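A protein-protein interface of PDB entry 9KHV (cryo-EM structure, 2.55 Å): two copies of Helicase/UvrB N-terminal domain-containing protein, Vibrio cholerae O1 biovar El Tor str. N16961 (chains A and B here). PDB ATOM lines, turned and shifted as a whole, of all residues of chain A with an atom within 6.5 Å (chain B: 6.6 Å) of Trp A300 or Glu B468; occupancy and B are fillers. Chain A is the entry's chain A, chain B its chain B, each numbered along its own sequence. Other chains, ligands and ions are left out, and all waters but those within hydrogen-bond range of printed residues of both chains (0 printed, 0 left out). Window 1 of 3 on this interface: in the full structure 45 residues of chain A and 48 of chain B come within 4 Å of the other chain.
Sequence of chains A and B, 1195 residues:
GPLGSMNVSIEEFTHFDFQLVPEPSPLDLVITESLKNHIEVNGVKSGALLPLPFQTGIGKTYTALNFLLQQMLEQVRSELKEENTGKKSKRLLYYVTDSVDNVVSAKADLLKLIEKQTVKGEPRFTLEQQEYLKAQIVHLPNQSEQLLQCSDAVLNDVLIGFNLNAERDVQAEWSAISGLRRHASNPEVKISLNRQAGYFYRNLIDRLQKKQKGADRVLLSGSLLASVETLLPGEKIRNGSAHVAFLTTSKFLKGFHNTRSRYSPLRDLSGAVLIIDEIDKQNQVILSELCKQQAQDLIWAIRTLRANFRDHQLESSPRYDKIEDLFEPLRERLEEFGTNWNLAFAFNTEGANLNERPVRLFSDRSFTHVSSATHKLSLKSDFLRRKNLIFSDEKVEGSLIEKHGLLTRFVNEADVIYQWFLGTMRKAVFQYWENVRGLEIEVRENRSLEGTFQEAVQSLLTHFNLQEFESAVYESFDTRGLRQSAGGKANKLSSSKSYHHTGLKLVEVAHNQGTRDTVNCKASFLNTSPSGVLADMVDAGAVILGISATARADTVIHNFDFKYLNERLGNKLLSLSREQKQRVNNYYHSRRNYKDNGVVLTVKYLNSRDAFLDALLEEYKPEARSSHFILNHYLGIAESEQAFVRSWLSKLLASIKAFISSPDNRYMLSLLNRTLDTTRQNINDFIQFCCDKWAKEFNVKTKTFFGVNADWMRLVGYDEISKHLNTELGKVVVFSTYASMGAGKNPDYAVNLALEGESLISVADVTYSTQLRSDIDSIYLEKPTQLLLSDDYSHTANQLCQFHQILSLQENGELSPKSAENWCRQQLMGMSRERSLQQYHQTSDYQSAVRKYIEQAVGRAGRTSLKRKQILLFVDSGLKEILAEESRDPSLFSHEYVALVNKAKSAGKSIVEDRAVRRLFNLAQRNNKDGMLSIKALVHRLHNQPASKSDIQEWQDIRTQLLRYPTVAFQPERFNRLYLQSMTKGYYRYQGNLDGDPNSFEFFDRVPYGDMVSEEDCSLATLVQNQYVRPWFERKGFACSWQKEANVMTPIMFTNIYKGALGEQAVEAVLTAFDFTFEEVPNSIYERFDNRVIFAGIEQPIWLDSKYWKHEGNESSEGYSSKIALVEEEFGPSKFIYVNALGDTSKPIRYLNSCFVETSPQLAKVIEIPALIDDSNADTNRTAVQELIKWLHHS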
ATOM      1  N   GLN A 296      22.701  -9.542 -20.983  1.00  0.00           N
ATOM      2  CA  GLN A 296      23.676 -10.605 -21.157  1.00  0.00           C
ATOM      3  C   GLN A 296      24.880 -10.362 -20.258  1.00  0.00           C
ATOM      4  O   GLN A 296      25.349  -9.227 -20.129  1.00  0.00           O
ATOM      5  CB  GLN A 296      24.126 -10.698 -22.618  1.00  0.00           C
ATOM      6  CG  GLN A 296      25.129 -11.804 -22.898  1.00  0.00           C
ATOM      7  CD  GLN A 296      24.507 -13.184 -22.843  1.00  0.00           C
ATOM      8  OE1 GLN A 296      23.950 -13.665 -23.826  1.00  0.00           O
ATOM      9  NE2 GLN A 296      24.597 -13.824 -21.687  1.00  0.00           N
ATOM     10  N   ASP A 297      25.374 -11.429 -19.637  1.00  0.00           N
ATOM     11  CA  ASP A 297      26.627 -11.380 -18.895  1.00  0.00           C
ATOM     12  C   ASP A 297      27.783 -11.503 -19.879  1.00  0.00           C
ATOM     13  O   ASP A 297      27.947 -12.542 -20.525  1.00  0.00           O
ATOM     14  CB  ASP A 297      26.673 -12.497 -17.855  1.00  0.00           C
ATOM     15  CG  ASP A 297      27.905 -12.429 -16.969  1.00  0.00           C
ATOM     16  OD1 ASP A 297      28.606 -11.397 -16.981  1.00  0.00           O
ATOM     17  OD2 ASP A 297      28.173 -13.413 -16.252  1.00  0.00           O
ATOM     18  N   LEU A 298      28.580 -10.441 -19.999  1.00  0.00           N
ATOM     19  CA  LEU A 298      29.615 -10.409 -21.026  1.00  0.00           C
ATOM     20  C   LEU A 298      30.782 -11.322 -20.677  1.00  0.00           C
ATOM     21  O   LEU A 298      31.361 -11.957 -21.564  1.00  0.00           O
ATOM     22  CB  LEU A 298      30.102  -8.977 -21.236  1.00  0.00           C
ATOM     23  CG  LEU A 298      29.253  -8.068 -22.124  1.00  0.00           C
ATOM     24  CD1 LEU A 298      29.927  -6.719 -22.283  1.00  0.00           C
ATOM     25  CD2 LEU A 298      29.006  -8.710 -23.474  1.00  0.00           C
ATOM     26  N   ILE A 299      31.147 -11.403 -19.397  1.00  0.00           N
ATOM     27  CA  ILE A 299      32.256 -12.266 -18.999  1.00  0.00           C
ATOM     28  C   ILE A 299      31.928 -13.721 -19.302  1.00  0.00           C
ATOM     29  O   ILE A 299      32.716 -14.437 -19.932  1.00  0.00           O
ATOM     30  CB  ILE A 299      32.592 -12.059 -17.511  1.00  0.00           C
ATOM     31  CG1 ILE A 299      33.147 -10.655 -17.280  1.00  0.00           C
ATOM     32  CG2 ILE A 299      33.586 -13.103 -17.042  1.00  0.00           C
ATOM     33  CD1 ILE A 299      33.207 -10.256 -15.833  1.00  0.00           C
ATOM     34  N   TRP A 300      30.742 -14.171 -18.883  1.00  0.00           N
ATOM     35  CA  TRP A 300      30.332 -15.545 -19.150  1.00  0.00           C
ATOM     36  C   TRP A 300      30.249 -15.818 -20.645  1.00  0.00           C
ATOM     37  O   TRP A 300      30.697 -16.869 -21.116  1.00  0.00           O
ATOM     38  CB  TRP A 300      28.987 -15.834 -18.483  1.00  0.00           C
ATOM     39  CG  TRP A 300      28.380 -17.125 -18.936  1.00  0.00           C
ATOM     40  CD1 TRP A 300      28.610 -18.363 -18.421  1.00  0.00           C
ATOM     41  CD2 TRP A 300      27.455 -17.306 -20.015  1.00  0.00           C
ATOM     42  NE1 TRP A 300      27.887 -19.304 -19.105  1.00  0.00           N
ATOM     43  CE2 TRP A 300      27.169 -18.681 -20.091  1.00  0.00           C
ATOM     44  CE3 TRP A 300      26.843 -16.440 -20.923  1.00  0.00           C
ATOM     45  CZ2 TRP A 300      26.296 -19.208 -21.035  1.00  0.00           C
ATOM     46  CZ3 TRP A 300      25.979 -16.965 -21.861  1.00  0.00           C
ATOM     47  CH2 TRP A 300      25.713 -18.335 -21.910  1.00  0.00           C
ATOM     48  N   ALA A 301      29.680 -14.882 -21.407  1.00  0.00           N
ATOM     49  CA  ALA A 301      29.493 -15.099 -22.837  1.00  0.00           C
ATOM     50  C   ALA A 301      30.828 -15.199 -23.561  1.00  0.00           C
ATOM     51  O   ALA A 301      31.035 -16.097 -24.386  1.00  0.00           O
ATOM     52  CB  ALA A 301      28.641 -13.977 -23.428  1.00  0.00           C
ATOM     53  N   ILE A 302      31.749 -14.283 -23.265  1.00  0.00           N
ATOM     54  CA  ILE A 302      33.038 -14.296 -23.946  1.00  0.00           C
ATOM     55  C   ILE A 302      33.851 -15.515 -23.529  1.00  0.00           C
ATOM     56  O   ILE A 302      34.530 -16.131 -24.358  1.00  0.00           O
ATOM     57  CB  ILE A 302      33.797 -12.983 -23.690  1.00  0.00           C
ATOM     58  CG1 ILE A 302      33.001 -11.803 -24.239  1.00  0.00           C
ATOM     59  CG2 ILE A 302      35.145 -13.009 -24.367  1.00  0.00           C
ATOM     60  CD1 ILE A 302      32.743 -11.885 -25.721  1.00  0.00           C
ATOM     61  N   ARG A 303      33.786 -15.897 -22.249  1.00  0.00           N
ATOM     62  CA  ARG A 303      34.503 -17.089 -21.809  1.00  0.00           C
ATOM     63  C   ARG A 303      33.954 -18.343 -22.478  1.00  0.00           C
ATOM     64  O   ARG A 303      34.721 -19.219 -22.893  1.00  0.00           O
ATOM     65  CB  ARG A 303      34.434 -17.212 -20.288  1.00  0.00           C
ATOM     66  CG  ARG A 303      35.466 -16.384 -19.551  1.00  0.00           C
ATOM     67  CD  ARG A 303      35.274 -16.469 -18.052  1.00  0.00           C
ATOM     68  NE  ARG A 303      36.341 -17.215 -17.399  1.00  0.00           N
ATOM     69  CZ  ARG A 303      36.220 -17.830 -16.231  1.00  0.00           C
ATOM     70  NH1 ARG A 303      35.084 -17.814 -15.556  1.00  0.00           N
ATOM     71  NH2 ARG A 303      37.265 -18.475 -15.727  1.00  0.00           N
ATOM     72  N   THR A 304      32.629 -18.440 -22.605  1.00  0.00           N
ATOM     73  CA  THR A 304      32.028 -19.589 -23.274  1.00  0.00           C
ATOM     74  C   THR A 304      32.411 -19.639 -24.746  1.00  0.00           C
ATOM     75  O   THR A 304      32.759 -20.705 -25.270  1.00  0.00           O
ATOM     76  CB  THR A 304      30.508 -19.540 -23.126  1.00  0.00           C
ATOM     77  OG1 THR A 304      30.170 -19.237 -21.769  1.00  0.00           O
ATOM     78  CG2 THR A 304      29.899 -20.863 -23.503  1.00  0.00           C
ATOM     79  N   LEU A 305      32.352 -18.496 -25.432  1.00  0.00           N
ATOM     80  CA  LEU A 305      32.726 -18.460 -26.841  1.00  0.00           C
ATOM     81  C   LEU A 305      34.184 -18.846 -27.035  1.00  0.00           C
ATOM     82  O   LEU A 305      34.516 -19.595 -27.959  1.00  0.00           O
ATOM     83  CB  LEU A 305      32.461 -17.071 -27.423  1.00  0.00           C
ATOM     84  CG  LEU A 305      31.003 -16.668 -27.634  1.00  0.00           C
ATOM     85  CD1 LEU A 305      30.908 -15.194 -27.976  1.00  0.00           C
ATOM     86  CD2 LEU A 305      30.364 -17.512 -28.715  1.00  0.00           C
ATOM     87  N   GLU A 468      23.471 -22.813 -25.625  1.00  0.00           N
ATOM     88  CA  GLU A 468      22.986 -21.859 -24.635  1.00  0.00           C
ATOM     89  C   GLU A 468      22.783 -20.460 -25.200  1.00  0.00           C
ATOM     90  O   GLU A 468      22.126 -19.642 -24.551  1.00  0.00           O
ATOM     91  CB  GLU A 468      23.952 -21.801 -23.454  1.00  0.00           C
ATOM     92  CG  GLU A 468      25.369 -21.438 -23.845  1.00  0.00           C
ATOM     93  CD  GLU A 468      26.197 -22.650 -24.212  1.00  0.00           C
ATOM     94  OE1 GLU A 468      25.639 -23.768 -24.238  1.00  0.00           O
ATOM     95  OE2 GLU A 468      27.402 -22.487 -24.481  1.00  0.00           O
ATOM     96  N   PHE A 469      23.325 -20.163 -26.379  1.00  0.00           N
ATOM     97  CA  PHE A 469      23.097 -18.893 -27.050  1.00  0.00           C
ATOM     98  C   PHE A 469      21.837 -18.912 -27.900  1.00  0.00           C
ATOM     99  O   PHE A 469      21.444 -17.868 -28.433  1.00  0.00           O
ATOM    100  CB  PHE A 469      24.305 -18.533 -27.915  1.00  0.00           C
ATOM    101  CG  PHE A 469      25.476 -18.025 -27.132  1.00  0.00           C
ATOM    102  CD1 PHE A 469      25.505 -16.722 -26.671  1.00  0.00           C
ATOM    103  CD2 PHE A 469      26.545 -18.852 -26.849  1.00  0.00           C
ATOM    104  CE1 PHE A 469      26.579 -16.257 -25.950  1.00  0.00           C
ATOM    105  CE2 PHE A 469      27.621 -18.390 -26.126  1.00  0.00           C
ATOM    106  CZ  PHE A 469      27.639 -17.093 -25.678  1.00  0.00           C
ATOM    107  N   GLN B 296      20.124 -36.332 -18.868  1.00  0.00           N
ATOM    108  CA  GLN B 296      21.260 -35.513 -19.256  1.00  0.00           C
ATOM    109  C   GLN B 296      21.781 -35.958 -20.615  1.00  0.00           C
ATOM    110  O   GLN B 296      21.868 -37.155 -20.894  1.00  0.00           O
ATOM    111  CB  GLN B 296      22.377 -35.602 -18.213  1.00  0.00           C
ATOM    112  CG  GLN B 296      23.600 -34.757 -18.527  1.00  0.00           C
ATOM    113  CD  GLN B 296      23.348 -33.276 -18.351  1.00  0.00           C
ATOM    114  OE1 GLN B 296      23.467 -32.740 -17.253  1.00  0.00           O
ATOM    115  NE2 GLN B 296      22.990 -32.606 -19.438  1.00  0.00           N
ATOM    116  N   TRP B 300      26.872 -33.411 -24.915  1.00  0.00           N
ATOM    117  CA  TRP B 300      26.956 -32.000 -24.558  1.00  0.00           C
ATOM    118  C   TRP B 300      27.679 -31.804 -23.234  1.00  0.00           C
ATOM    119  O   TRP B 300      28.514 -30.903 -23.106  1.00  0.00           O
ATOM    120  CB  TRP B 300      25.557 -31.387 -24.493  1.00  0.00           C
ATOM    121  CG  TRP B 300      25.546 -30.026 -23.872  1.00  0.00           C
ATOM    122  CD1 TRP B 300      25.755 -28.837 -24.500  1.00  0.00           C
ATOM    123  CD2 TRP B 300      25.334 -29.715 -22.489  1.00  0.00           C
ATOM    124  NE1 TRP B 300      25.684 -27.806 -23.601  1.00  0.00           N
ATOM    125  CE2 TRP B 300      25.427 -28.318 -22.358  1.00  0.00           C
ATOM    126  CE3 TRP B 300      25.077 -30.483 -21.351  1.00  0.00           C
ATOM    127  CZ2 TRP B 300      25.269 -27.674 -21.137  1.00  0.00           C
ATOM    128  CZ3 TRP B 300      24.922 -29.842 -20.141  1.00  0.00           C
ATOM    129  CH2 TRP B 300      25.018 -28.452 -20.042  1.00  0.00           C
ATOM    130  N   THR B 304      31.211 -29.870 -22.849  1.00  0.00           N
ATOM    131  CA  THR B 304      31.281 -28.664 -22.031  1.00  0.00           C
ATOM    132  C   THR B 304      32.345 -28.786 -20.948  1.00  0.00           C
ATOM    133  O   THR B 304      33.128 -27.853 -20.733  1.00  0.00           O
ATOM    134  CB  THR B 304      29.918 -28.380 -21.402  1.00  0.00           C
ATOM    135  OG1 THR B 304      28.896 -28.511 -22.395  1.00  0.00           O
ATOM    136  CG2 THR B 304      29.875 -26.986 -20.822  1.00  0.00           C
ATOM    137  N   ASN B 308      35.687 -26.398 -20.806  1.00  0.00           N
ATOM    138  CA  ASN B 308      35.830 -25.442 -19.718  1.00  0.00           C
ATOM    139  C   ASN B 308      36.897 -25.819 -18.700  1.00  0.00           C
ATOM    140  O   ASN B 308      37.404 -24.933 -18.008  1.00  0.00           O
ATOM    141  CB  ASN B 308      34.489 -25.253 -19.008  1.00  0.00           C
ATOM    142  CG  ASN B 308      33.538 -24.383 -19.796  1.00  0.00           C
ATOM    143  OD1 ASN B 308      33.721 -23.173 -19.892  1.00  0.00           O
ATOM    144  ND2 ASN B 308      32.526 -25.000 -20.383  1.00  0.00           N
ATOM    145  N   LEU B 461      31.290 -23.040  -9.429  1.00  0.00           N
ATOM    146  CA  LEU B 461      30.789 -23.116 -10.793  1.00  0.00           C
ATOM    147  C   LEU B 461      31.061 -21.847 -11.588  1.00  0.00           C
ATOM    148  O   LEU B 461      31.217 -21.919 -12.809  1.00  0.00           O
ATOM    149  CB  LEU B 461      29.294 -23.428 -10.782  1.00  0.00           C
ATOM    150  CG  LEU B 461      28.953 -24.880 -10.441  1.00  0.00           C
ATOM    151  CD1 LEU B 461      27.478 -25.119 -10.601  1.00  0.00           C
ATOM    152  CD2 LEU B 461      29.750 -25.857 -11.287  1.00  0.00           C
ATOM    153  N   ASN B 465      33.344 -21.504 -14.921  1.00  0.00           N
ATOM    154  CA  ASN B 465      32.462 -21.150 -16.033  1.00  0.00           C
ATOM    155  C   ASN B 465      31.523 -22.306 -16.378  1.00  0.00           C
ATOM    156  O   ASN B 465      31.211 -22.554 -17.543  1.00  0.00           O
ATOM    157  CB  ASN B 465      33.272 -20.706 -17.255  1.00  0.00           C
ATOM    158  CG  ASN B 465      32.442 -19.969 -18.283  1.00  0.00           C
ATOM    159  OD1 ASN B 465      31.845 -18.937 -17.991  1.00  0.00           O
ATOM    160  ND2 ASN B 465      32.406 -20.498 -19.498  1.00  0.00           N
ATOM    161  N   LEU B 466      31.062 -23.014 -15.350  1.00  0.00           N
ATOM    162  CA  LEU B 466      30.246 -24.212 -15.501  1.00  0.00           C
ATOM    163  C   LEU B 466      28.882 -24.038 -14.846  1.00  0.00           C
ATOM    164  O   LEU B 466      28.337 -24.968 -14.253  1.00  0.00           O
ATOM    165  CB  LEU B 466      30.962 -25.430 -14.925  1.00  0.00           C
ATOM    166  CG  LEU B 466      32.114 -26.010 -15.745  1.00  0.00           C
ATOM    167  CD1 LEU B 466      32.920 -26.984 -14.915  1.00  0.00           C
ATOM    168  CD2 LEU B 466      31.593 -26.687 -16.997  1.00  0.00           C
ATOM    169  N   GLN B 467      28.303 -22.842 -14.965  1.00  0.00           N
ATOM    170  CA  GLN B 467      27.047 -22.540 -14.289  1.00  0.00           C
ATOM    171  C   GLN B 467      25.886 -23.396 -14.781  1.00  0.00           C
ATOM    172  O   GLN B 467      24.930 -23.611 -14.026  1.00  0.00           O
ATOM    173  CB  GLN B 467      26.708 -21.059 -14.460  1.00  0.00           C
ATOM    174  CG  GLN B 467      27.667 -20.114 -13.756  1.00  0.00           C
ATOM    175  CD  GLN B 467      28.676 -19.496 -14.703  1.00  0.00           C
ATOM    176  OE1 GLN B 467      29.046 -20.095 -15.708  1.00  0.00           O
ATOM    177  NE2 GLN B 467      29.124 -18.288 -14.385  1.00  0.00           N
ATOM    178  N   GLU B 468      25.950 -23.899 -16.015  1.00  0.00           N
ATOM    179  CA  GLU B 468      24.863 -24.694 -16.574  1.00  0.00           C
ATOM    180  C   GLU B 468      24.642 -26.004 -15.831  1.00  0.00           C
ATOM    181  O   GLU B 468      23.567 -26.596 -15.968  1.00  0.00           O
ATOM    182  CB  GLU B 468      25.128 -24.993 -18.049  1.00  0.00           C
ATOM    183  CG  GLU B 468      25.873 -23.901 -18.790  1.00  0.00           C
ATOM    184  CD  GLU B 468      27.377 -24.046 -18.676  1.00  0.00           C
ATOM    185  OE1 GLU B 468      27.870 -25.188 -18.783  1.00  0.00           O
ATOM    186  OE2 GLU B 468      28.063 -23.020 -18.478  1.00  0.00           O
ATOM    187  N   PHE B 469      25.620 -26.468 -15.061  1.00  0.00           N
ATOM    188  CA  PHE B 469      25.488 -27.675 -14.262  1.00  0.00           C
ATOM    189  C   PHE B 469      24.882 -27.402 -12.895  1.00  0.00           C
ATOM    190  O   PHE B 469      24.701 -28.341 -12.113  1.00  0.00           O
ATOM    191  CB  PHE B 469      26.852 -28.345 -14.104  1.00  0.00           C
ATOM    192  CG  PHE B 469      27.333 -29.030 -15.346  1.00  0.00           C
ATOM    193  CD1 PHE B 469      26.839 -30.270 -15.703  1.00  0.00           C
ATOM    194  CD2 PHE B 469      28.268 -28.428 -16.164  1.00  0.00           C
ATOM    195  CE1 PHE B 469      27.278 -30.897 -16.848  1.00  0.00           C
ATOM    196  CE2 PHE B 469      28.708 -29.052 -17.311  1.00  0.00           C
ATOM    197  CZ  PHE B 469      28.213 -30.287 -17.651  1.00  0.00           C
ATOM    198  N   GLU B 470      24.550 -26.138 -12.609  1.00  0.00           N
ATOM    199  CA  GLU B 470      24.076 -25.747 -11.284  1.00  0.00           C
ATOM    200  C   GLU B 470      22.979 -26.673 -10.781  1.00  0.00           C
ATOM    201  O   GLU B 470      23.160 -27.382  -9.784  1.00  0.00           O
ATOM    202  CB  GLU B 470      23.597 -24.296 -11.327  1.00  0.00           C
ATOM    203  CG  GLU B 470      23.576 -23.593  -9.986  1.00  0.00           C
ATOM    204  CD  GLU B 470      22.389 -22.661  -9.846  1.00  0.00           C
ATOM    205  OE1 GLU B 470      22.529 -21.469 -10.188  1.00  0.00           O
ATOM    206  OE2 GLU B 470      21.312 -23.121  -9.416  1.00  0.00           O
ATOM    207  N   SER B 471      21.845 -26.714 -11.485  1.00  0.00           N
ATOM    208  CA  SER B 471      20.762 -27.598 -11.076  1.00  0.00           C
ATOM    209  C   SER B 471      21.235 -29.042 -10.995  1.00  0.00           C
ATOM    210  O   SER B 471      20.958 -29.735 -10.009  1.00  0.00           O
ATOM    211  CB  SER B 471      19.587 -27.473 -12.043  1.00  0.00           C
ATOM    212  OG  SER B 471      20.039 -27.400 -13.383  1.00  0.00           O
ATOM    213  N   ALA B 472      21.992 -29.493 -11.998  1.00  0.00           N
ATOM    214  CA  ALA B 472      22.455 -30.876 -12.010  1.00  0.00           C
ATOM    215  C   ALA B 472      23.281 -31.189 -10.772  1.00  0.00           C
ATOM    216  O   ALA B 472      23.288 -32.328 -10.292  1.00  0.00           O
ATOM    217  CB  ALA B 472      23.261 -31.151 -13.278  1.00  0.00           C
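Of the 12 printed residues of chain A, 3 touch a printed residue of chain B.
Printed residues of chain A that touch a printed residue of chain B: Trp A300, Arg A303 and Thr A304.
O of Trp A300 lies within hydrogen-bond range of OG1 of Thr A304 (2.5 Å).
The side-chain amide oxygen (OD1) of Asn B308 sits at hydrogen-bond distance from the side-chain amide nitrogen (ND2) of Asn B465, at 3.0 Å.
Trp A300 touches Glu B468, but with the chains exchanged Glu A468 does not touch Trp B300 (4.1 Å).
Positions printed for both chains: 296, 300, 304, 468 and 469.
Glu B468 touches just one residue of chain A: Trp A300 (3.8 Å).
Of the printed residues of chain B, Arg A303 touches Asn B465.
Of the printed residues of chain B, Thr A304 touches Asn B465.
Of the printed residues of chain A, Asn B465 touches Trp A300 (3.3 Å), Arg A303 (3.8 Å) and Thr A304 (3.4 Å).
Thr B304 touches none of the printed residues of chain A.
Trp B300 touches none of the printed residues of chain A.
The nearest residue of chain B that does not touch Trp A300 is Leu B466 (6.1 Å).
Asn B465 touches Trp A300.
Gln B467 touches Trp A300.
Trp A300 touches Glu B468.
NH1 of Arg A303 touches CB of Asn B465, 3.8 Å away.
The side-chain hydroxyl (OG1) of Thr A304 is in hydrogen-bond range of the side-chain amide nitrogen (ND2) of Asn B465, at 3.4 Å.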
